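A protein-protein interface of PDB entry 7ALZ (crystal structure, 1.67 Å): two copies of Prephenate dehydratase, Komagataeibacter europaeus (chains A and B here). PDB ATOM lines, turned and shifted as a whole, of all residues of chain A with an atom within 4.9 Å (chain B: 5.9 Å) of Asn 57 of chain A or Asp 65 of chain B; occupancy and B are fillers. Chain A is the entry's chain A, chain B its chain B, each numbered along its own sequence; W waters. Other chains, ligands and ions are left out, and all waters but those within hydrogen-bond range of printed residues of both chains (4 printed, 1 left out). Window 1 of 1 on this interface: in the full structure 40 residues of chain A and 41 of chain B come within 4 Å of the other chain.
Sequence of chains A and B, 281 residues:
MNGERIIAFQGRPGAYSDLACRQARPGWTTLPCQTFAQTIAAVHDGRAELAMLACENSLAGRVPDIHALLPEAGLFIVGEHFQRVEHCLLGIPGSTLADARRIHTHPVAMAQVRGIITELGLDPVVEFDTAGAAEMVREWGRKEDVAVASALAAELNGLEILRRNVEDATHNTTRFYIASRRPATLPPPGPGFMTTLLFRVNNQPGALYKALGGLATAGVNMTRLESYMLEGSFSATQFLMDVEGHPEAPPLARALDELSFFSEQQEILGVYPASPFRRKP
O of Ser 58 of chain A is in hydrogen-bond range of NE2 of His 67 of chain B. N of Asp 65 of chain B lies within hydrogen-bond range of O of Gly 61 of chain A. OD2 of Asp 65 of chain B sits close to O of Asn 57 of chain A (3.4 Å).
The side-chain amide oxygen of Asn 57 of chain A sits at hydrogen-bond distance from the side-chain hydroxyl of Thr 174 of chain A, at 2.7 Å. The side-chain hydroxyl (OG) of Ser 58 of chain A sits at hydrogen-bond distance from the backbone NH (N) of Thr 173 of chain A (3.0 Å). The side-chain carboxylate of Asp 65 of chain B lies within hydrogen-bond range of a ring nitrogen (ND1) of His 67 of chain B (2.5 Å). OD1 of Asn 57 of chain A is in hydrogen-bond range of ND2 of Asn 172 of chain A (2.9 Å). The backbone carbonyl oxygen (O) of Ala 60 of chain A sits close to the side-chain amide oxygen (OD1) of Asn 57 of chain A. The backbone NH (N) of Ala 60 of chain A lies within hydrogen-bond range of the side-chain amide oxygen (OD1) of Asn 172 of chain A (3.2 Å).
Glu 56 of chain A touches Met 229 of chain B. O of Asn 57 of chain A touches CE1 of His 67 of chain B, 3.6 Å away. Met 229 of chain B touches Asn 57 of chain A (CE to C, 3.7 Å). Ser 58 of chain A touches Met 229 of chain B (N to CE, 3.5 Å). Leu 59 of chain A touches Ala 68 of chain B. Leu 69 of chain B touches Ala 60 of chain A. Gly 61 of chain A touches Val 63 of chain B (O to O, 3.9 Å). CA of Pro 64 of chain B touches O of Gly 61 of chain A (3.8 Å). Val 63 of chain B touches Arg 62 of chain A. Thr 173 of chain A touches Met 229 of chain B (O to CE, 3.3 Å).
Printed residues of chain B within 4 Å of Glu 56 of chain A: Met 229 (3.6 Å). Of chain B, only Asp 65, His 67 and Met 229 come within 4 Å of Asn 57 of chain A. Printed residues of chain B within 4 Å of Ser 58 of chain A: His 67 (3.1 Å) and Met 229 (3.5 Å). Printed residues of chain A within 4 Å of Asp 65 of chain B: Asn 57 and Gly 61. Ile 66 of chain B touches none of the printed residues of chain A. Of the printed residues of chain A, His 67 of chain B touches Asn 57 (3.6 Å) and Ser 58 (3.1 Å). The nearest residue of chain A that does not touch Asp 65 of chain B is Leu 59 of chain A (4.5 Å). The nearest printed residue of chain A that does not touch Ala 68 of chain B is Ser 58 of chain A (4.8 Å).
Printed residues of chain B that touch a printed residue of chain A: Val 63, Pro 64, Asp 65, His 67, Ala 68, Leu 69 and Met 229. Hydrophobic or aromatic side chains of chain B within 4 Å of the printed part of chain A: His 67, Ala 68, Leu 69 and Met 229. Along chain B the printed residues that touch a printed residue of chain A span positions 63 to 229. Among the printed residues, no Asp or Glu carboxylate lies within 4 Å of a Lys or Arg side-chain nitrogen of the other chain.
Position printed for both chains: 63. Of the 13 pairs that touch across the chains among the printed residues, none has its exchanged pair printed and touching as well.
Water W1 lies within hydrogen-bond range of the side-chain carboxylate of Asp 65 of chain B (2.6 Å) and the backbone NH of Asn 57 of chain A (2.8 Å). Water W4 lies within hydrogen-bond range of O of Asp 65 of chain B (2.7 Å) and N of Gly 61 of chain A (3.1 Å). Water W2 lies within hydrogen-bond range of O of Val 63 of chain B, N of Val 63 of chain A and O of Gly 61 of chain A. Water W3 bridges O of Asn 57 of chain A (2.9 Å) and N of Met 229 of chain B (2.9 Å).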
ATOM      1  N   CYS A  55      25.386  -2.292 -25.505  1.00  0.00           N
ATOM      2  CA  CYS A  55      26.288  -1.962 -24.391  1.00  0.00           C
ATOM      3  C   CYS A  55      26.052  -0.661 -23.657  1.00  0.00           C
ATOM      4  O   CYS A  55      26.396  -0.563 -22.505  1.00  0.00           O
ATOM      5  CB  CYS A  55      27.752  -2.074 -24.772  1.00  0.00           C
ATOM      6  SG  CYS A  55      28.269  -0.927 -26.057  1.00  0.00           S
ATOM      7  N   GLU A  56      25.502   0.330 -24.349  1.00  0.00           N
ATOM      8  CA  GLU A  56      25.192   1.650 -23.757  1.00  0.00           C
ATOM      9  C   GLU A  56      23.966   2.262 -24.371  1.00  0.00           C
ATOM     10  O   GLU A  56      23.666   2.047 -25.547  1.00  0.00           O
ATOM     11  CB  GLU A  56      26.390   2.582 -23.897  1.00  0.00           C
ATOM     12  CG  GLU A  56      27.699   2.110 -23.300  1.00  0.00           C
ATOM     13  CD  GLU A  56      28.771   3.188 -23.327  1.00  0.00           C
ATOM     14  OE1 GLU A  56      28.659   4.094 -22.454  1.00  0.00           O
ATOM     15  OE2 GLU A  56      29.653   3.231 -24.248  1.00  0.00           O
ATOM     16  N   ASN A  57      23.236   3.072 -23.560  1.00  0.00           N
ATOM     17  CA  ASN A  57      22.149   3.888 -24.107  1.00  0.00           C
ATOM     18  C   ASN A  57      22.283   5.311 -23.596  1.00  0.00           C
ATOM     19  O   ASN A  57      22.632   5.516 -22.433  1.00  0.00           O
ATOM     20  CB  ASN A  57      20.781   3.341 -23.733  1.00  0.00           C
ATOM     21  CG  ASN A  57      20.435   2.104 -24.485  1.00  0.00           C
ATOM     22  OD1 ASN A  57      20.001   2.171 -25.625  1.00  0.00           O
ATOM     23  ND2 ASN A  57      20.559   0.948 -23.813  1.00  0.00           N
ATOM     24  N   SER A  58      22.021   6.291 -24.458  1.00  0.00           N
ATOM     25  CA  SER A  58      22.122   7.677 -24.034  1.00  0.00           C
ATOM     26  C   SER A  58      20.983   8.142 -23.123  1.00  0.00           C
ATOM     27  O   SER A  58      21.166   9.079 -22.383  1.00  0.00           O
ATOM     28  CB  SER A  58      22.195   8.609 -25.241  1.00  0.00           C
ATOM     29  OG  SER A  58      20.990   8.565 -25.935  1.00  0.00           O
ATOM     30  N   LEU A  59      19.801   7.539 -23.239  1.00  0.00           N
ATOM     31  CA  LEU A  59      18.668   7.992 -22.457  1.00  0.00           C
ATOM     32  C   LEU A  59      18.140   6.895 -21.551  1.00  0.00           C
ATOM     33  O   LEU A  59      17.958   7.098 -20.330  1.00  0.00           O
ATOM     34  CB  LEU A  59      17.582   8.496 -23.413  1.00  0.00           C
ATOM     35  CG  LEU A  59      16.219   8.920 -22.845  1.00  0.00           C
ATOM     36  CD1 LEU A  59      16.374  10.112 -21.891  1.00  0.00           C
ATOM     37  CD2 LEU A  59      15.324   9.270 -24.001  1.00  0.00           C
ATOM     38  N   ALA A  60      17.846   5.736 -22.147  1.00  0.00           N
ATOM     39  CA  ALA A  60      17.200   4.659 -21.407  1.00  0.00           C
ATOM     40  C   ALA A  60      17.414   3.314 -22.090  1.00  0.00           C
ATOM     41  O   ALA A  60      17.605   3.232 -23.307  1.00  0.00           O
ATOM     42  CB  ALA A  60      15.733   4.948 -21.223  1.00  0.00           C
ATOM     43  N   GLY A  61      17.431   2.267 -21.255  1.00  0.00           N
ATOM     44  CA  GLY A  61      17.715   0.930 -21.720  1.00  0.00           C
ATOM     45  C   GLY A  61      18.181   0.051 -20.594  1.00  0.00           C
ATOM     46  O   GLY A  61      18.373   0.525 -19.454  1.00  0.00           O
ATOM     47  N   ARG A  62      18.224  -1.250 -20.887  1.00  0.00           N
ATOM     48  CA  ARG A  62      18.781  -2.298 -20.030  1.00  0.00           C
ATOM     49  C   ARG A  62      19.720  -2.981 -21.008  1.00  0.00           C
ATOM     50  O   ARG A  62      19.326  -3.362 -22.107  1.00  0.00           O
ATOM     51  CB  ARG A  62      17.696  -3.318 -19.639  1.00  0.00           C
ATOM     52  CG  ARG A  62      16.810  -2.933 -18.480  1.00  0.00           C
ATOM     53  CD  ARG A  62      15.420  -3.564 -18.570  1.00  0.00           C
ATOM     54  NE  ARG A  62      15.417  -5.014 -18.385  1.00  0.00           N
ATOM     55  CZ  ARG A  62      15.603  -5.629 -17.215  1.00  0.00           C
ATOM     56  NH1 ARG A  62      15.850  -4.926 -16.099  1.00  0.00           N
ATOM     57  NH2 ARG A  62      15.587  -6.951 -17.168  1.00  0.00           N
ATOM     58  N   VAL A  63      20.986  -3.072 -20.648  1.00  0.00           N
ATOM     59  CA  VAL A  63      21.952  -3.801 -21.474  1.00  0.00           C
ATOM     60  C   VAL A  63      22.496  -4.948 -20.637  1.00  0.00           C
ATOM     61  O   VAL A  63      22.523  -4.885 -19.419  1.00  0.00           O
ATOM     62  CB  VAL A  63      23.107  -2.910 -21.973  1.00  0.00           C
ATOM     63  CG1 VAL A  63      22.551  -1.846 -22.893  1.00  0.00           C
ATOM     64  CG2 VAL A  63      23.819  -2.265 -20.816  1.00  0.00           C
ATOM     65  N   ASN A 172      16.848   8.309 -28.455  1.00  0.00           N
ATOM     66  CA  ASN A 172      17.804   7.527 -27.680  1.00  0.00           C
ATOM     67  C   ASN A 172      18.838   7.003 -28.662  1.00  0.00           C
ATOM     68  O   ASN A 172      18.483   6.686 -29.799  1.00  0.00           O
ATOM     69  CB  ASN A 172      17.102   6.382 -26.963  1.00  0.00           C
ATOM     70  CG  ASN A 172      18.058   5.475 -26.215  1.00  0.00           C
ATOM     71  OD1 ASN A 172      18.688   5.862 -25.224  1.00  0.00           O
ATOM     72  ND2 ASN A 172      18.228   4.232 -26.750  1.00  0.00           N
ATOM     73  N   THR A 173      20.099   6.942 -28.238  1.00  0.00           N
ATOM     74  CA  THR A 173      21.146   6.303 -29.041  1.00  0.00           C
ATOM     75  C   THR A 173      21.530   5.006 -28.313  1.00  0.00           C
ATOM     76  O   THR A 173      21.874   5.040 -27.144  1.00  0.00           O
ATOM     77  CB  THR A 173      22.378   7.233 -29.205  1.00  0.00           C
ATOM     78  OG1 THR A 173      21.988   8.456 -29.854  1.00  0.00           O
ATOM     79  CG2 THR A 173      23.451   6.538 -30.016  1.00  0.00           C
ATOM     80  N   THR A 174      21.525   3.872 -29.030  1.00  0.00           N
ATOM     81  CA  THR A 174      22.008   2.620 -28.484  1.00  0.00           C
ATOM     82  C   THR A 174      23.383   2.342 -29.138  1.00  0.00           C
ATOM     83  O   THR A 174      23.525   2.405 -30.383  1.00  0.00           O
ATOM     84  CB  THR A 174      21.072   1.428 -28.737  1.00  0.00           C
ATOM     85  OG1 THR A 174      19.764   1.750 -28.305  1.00  0.00           O
ATOM     86  CG2 THR A 174      21.559   0.142 -28.100  1.00  0.00           C
ATOM     87  N   PHE B  36      10.631   0.107 -15.814  1.00  0.00           N
ATOM     88  CA  PHE B  36      11.399   1.038 -15.046  1.00  0.00           C
ATOM     89  C   PHE B  36      10.693   2.409 -14.895  1.00  0.00           C
ATOM     90  O   PHE B  36      10.548   2.926 -13.795  1.00  0.00           O
ATOM     91  CB  PHE B  36      12.798   1.189 -15.691  1.00  0.00           C
ATOM     92  CG  PHE B  36      13.634   2.252 -15.056  1.00  0.00           C
ATOM     93  CD1 PHE B  36      14.023   2.160 -13.734  1.00  0.00           C
ATOM     94  CD2 PHE B  36      14.049   3.350 -15.782  1.00  0.00           C
ATOM     95  CE1 PHE B  36      14.815   3.156 -13.140  1.00  0.00           C
ATOM     96  CE2 PHE B  36      14.864   4.326 -15.195  1.00  0.00           C
ATOM     97  CZ  PHE B  36      15.219   4.243 -13.865  1.00  0.00           C
ATOM     98  N   VAL B  63      20.301  -4.266 -15.827  1.00  0.00           N
ATOM     99  CA  VAL B  63      19.765  -3.301 -14.856  1.00  0.00           C
ATOM    100  C   VAL B  63      19.323  -2.086 -15.639  1.00  0.00           C
ATOM    101  O   VAL B  63      19.850  -1.799 -16.716  1.00  0.00           O
ATOM    102  CB  VAL B  63      20.806  -2.893 -13.771  1.00  0.00           C
ATOM    103  CG1 VAL B  63      21.236  -4.144 -12.984  1.00  0.00           C
ATOM    104  CG2 VAL B  63      22.033  -2.236 -14.348  1.00  0.00           C
ATOM    105  N   PRO B  64      18.357  -1.309 -15.104  1.00  0.00           N
ATOM    106  CA  PRO B  64      17.967  -0.061 -15.742  1.00  0.00           C
ATOM    107  C   PRO B  64      19.061   0.953 -15.632  1.00  0.00           C
ATOM    108  O   PRO B  64      19.810   1.036 -14.670  1.00  0.00           O
ATOM    109  CB  PRO B  64      16.743   0.373 -14.918  1.00  0.00           C
ATOM    110  CG  PRO B  64      17.005  -0.210 -13.556  1.00  0.00           C
ATOM    111  CD  PRO B  64      17.646  -1.561 -13.840  1.00  0.00           C
ATOM    112  N   ASP B  65      19.162   1.760 -16.678  1.00  0.00           N
ATOM    113  CA  ASP B  65      20.060   2.858 -16.686  1.00  0.00           C
ATOM    114  C   ASP B  65      19.315   4.073 -16.096  1.00  0.00           C
ATOM    115  O   ASP B  65      18.342   4.544 -16.698  1.00  0.00           O
ATOM    116  CB  ASP B  65      20.434   3.122 -18.127  1.00  0.00           C
ATOM    117  CG  ASP B  65      21.414   4.238 -18.268  1.00  0.00           C
ATOM    118  OD1 ASP B  65      21.496   5.056 -17.351  1.00  0.00           O
ATOM    119  OD2 ASP B  65      22.065   4.329 -19.331  1.00  0.00           O
ATOM    120  N   ILE B  66      19.790   4.546 -14.944  1.00  0.00           N
ATOM    121  CA  ILE B  66      19.186   5.606 -14.162  1.00  0.00           C
ATOM    122  C   ILE B  66      19.721   7.010 -14.367  1.00  0.00           C
ATOM    123  O   ILE B  66      19.170   7.928 -13.810  1.00  0.00           O
ATOM    124  CB  ILE B  66      19.286   5.347 -12.638  1.00  0.00           C
ATOM    125  CG1 ILE B  66      20.743   5.497 -12.127  1.00  0.00           C
ATOM    126  CG2 ILE B  66      18.623   4.004 -12.306  1.00  0.00           C
ATOM    127  CD1 ILE B  66      20.900   5.603 -10.629  1.00  0.00           C
ATOM    128  N   HIS B  67      20.797   7.166 -15.159  1.00  0.00           N
ATOM    129  CA  HIS B  67      21.553   8.424 -15.170  1.00  0.00           C
ATOM    130  C   HIS B  67      20.708   9.666 -15.555  1.00  0.00           C
ATOM    131  O   HIS B  67      20.873  10.753 -14.991  1.00  0.00           O
ATOM    132  CB  HIS B  67      22.848   8.301 -16.020  1.00  0.00           C
ATOM    133  CG  HIS B  67      22.679   8.370 -17.493  1.00  0.00           C
ATOM    134  ND1 HIS B  67      22.307   7.284 -18.253  1.00  0.00           N
ATOM    135  CD2 HIS B  67      22.880   9.378 -18.363  1.00  0.00           C
ATOM    136  CE1 HIS B  67      22.266   7.633 -19.528  1.00  0.00           C
ATOM    137  NE2 HIS B  67      22.600   8.907 -19.622  1.00  0.00           N
ATOM    138  N   ALA B  68      19.766   9.458 -16.468  1.00  0.00           N
ATOM    139  CA  ALA B  68      18.875  10.544 -16.957  1.00  0.00           C
ATOM    140  C   ALA B  68      17.501  10.556 -16.252  1.00  0.00           C
ATOM    141  O   ALA B  68      17.023  11.560 -15.761  1.00  0.00           O
ATOM    142  CB  ALA B  68      18.732  10.417 -18.459  1.00  0.00           C
ATOM    143  N   LEU B  69      16.870   9.391 -16.161  1.00  0.00           N
ATOM    144  CA  LEU B  69      15.447   9.366 -15.779  1.00  0.00           C
ATOM    145  C   LEU B  69      15.261   9.557 -14.294  1.00  0.00           C
ATOM    146  O   LEU B  69      14.232  10.136 -13.828  1.00  0.00           O
ATOM    147  CB  LEU B  69      14.774   8.104 -16.263  1.00  0.00           C
ATOM    148  CG  LEU B  69      14.751   7.920 -17.783  1.00  0.00           C
ATOM    149  CD1 LEU B  69      13.994   6.631 -18.081  1.00  0.00           C
ATOM    150  CD2 LEU B  69      14.180   9.079 -18.584  1.00  0.00           C
ATOM    151  N   TYR B 228      28.578   7.296 -18.942  1.00  0.00           N
ATOM    152  CA  TYR B 228      27.436   7.285 -19.850  1.00  0.00           C
ATOM    153  C   TYR B 228      27.617   8.296 -20.976  1.00  0.00           C
ATOM    154  O   TYR B 228      28.307   9.316 -20.823  1.00  0.00           O
ATOM    155  CB  TYR B 228      26.156   7.667 -19.087  1.00  0.00           C
ATOM    156  CG  TYR B 228      25.907   6.780 -17.936  1.00  0.00           C
ATOM    157  CD1 TYR B 228      25.196   5.595 -18.099  1.00  0.00           C
ATOM    158  CD2 TYR B 228      26.350   7.144 -16.670  1.00  0.00           C
ATOM    159  CE1 TYR B 228      24.985   4.752 -17.017  1.00  0.00           C
ATOM    160  CE2 TYR B 228      26.135   6.304 -15.582  1.00  0.00           C
ATOM    161  CZ  TYR B 228      25.435   5.142 -15.765  1.00  0.00           C
ATOM    162  OH  TYR B 228      25.216   4.271 -14.673  1.00  0.00           O
ATOM    163  N   MET B 229      27.028   7.954 -22.115  1.00  0.00           N
ATOM    164  CA  MET B 229      26.962   8.811 -23.286  1.00  0.00           C
ATOM    165  C   MET B 229      25.928   9.891 -23.054  1.00  0.00           C
ATOM    166  O   MET B 229      24.847   9.617 -22.535  1.00  0.00           O
ATOM    167  CB  MET B 229      26.543   7.996 -24.512  1.00  0.00           C
ATOM    168  CG  MET B 229      27.412   6.781 -24.714  1.00  0.00           C
ATOM    169  SD  MET B 229      26.937   5.869 -26.370  1.00  0.00           S
ATOM    170  CE  MET B 229      25.016   5.364 -26.089  1.00  0.00           C
HETATM  171  O   HOH W   1      23.618   2.748 -20.772  1.00  0.00           O
HETATM  172  O   HOH W   2      21.407  -0.818 -18.703  1.00  0.00           O
HETATM  173  O   HOH W   3      25.437   5.499 -21.924  1.00  0.00           O
HETATM  174  O   HOH W   4      16.762   3.170 -18.324  1.00  0.00           O
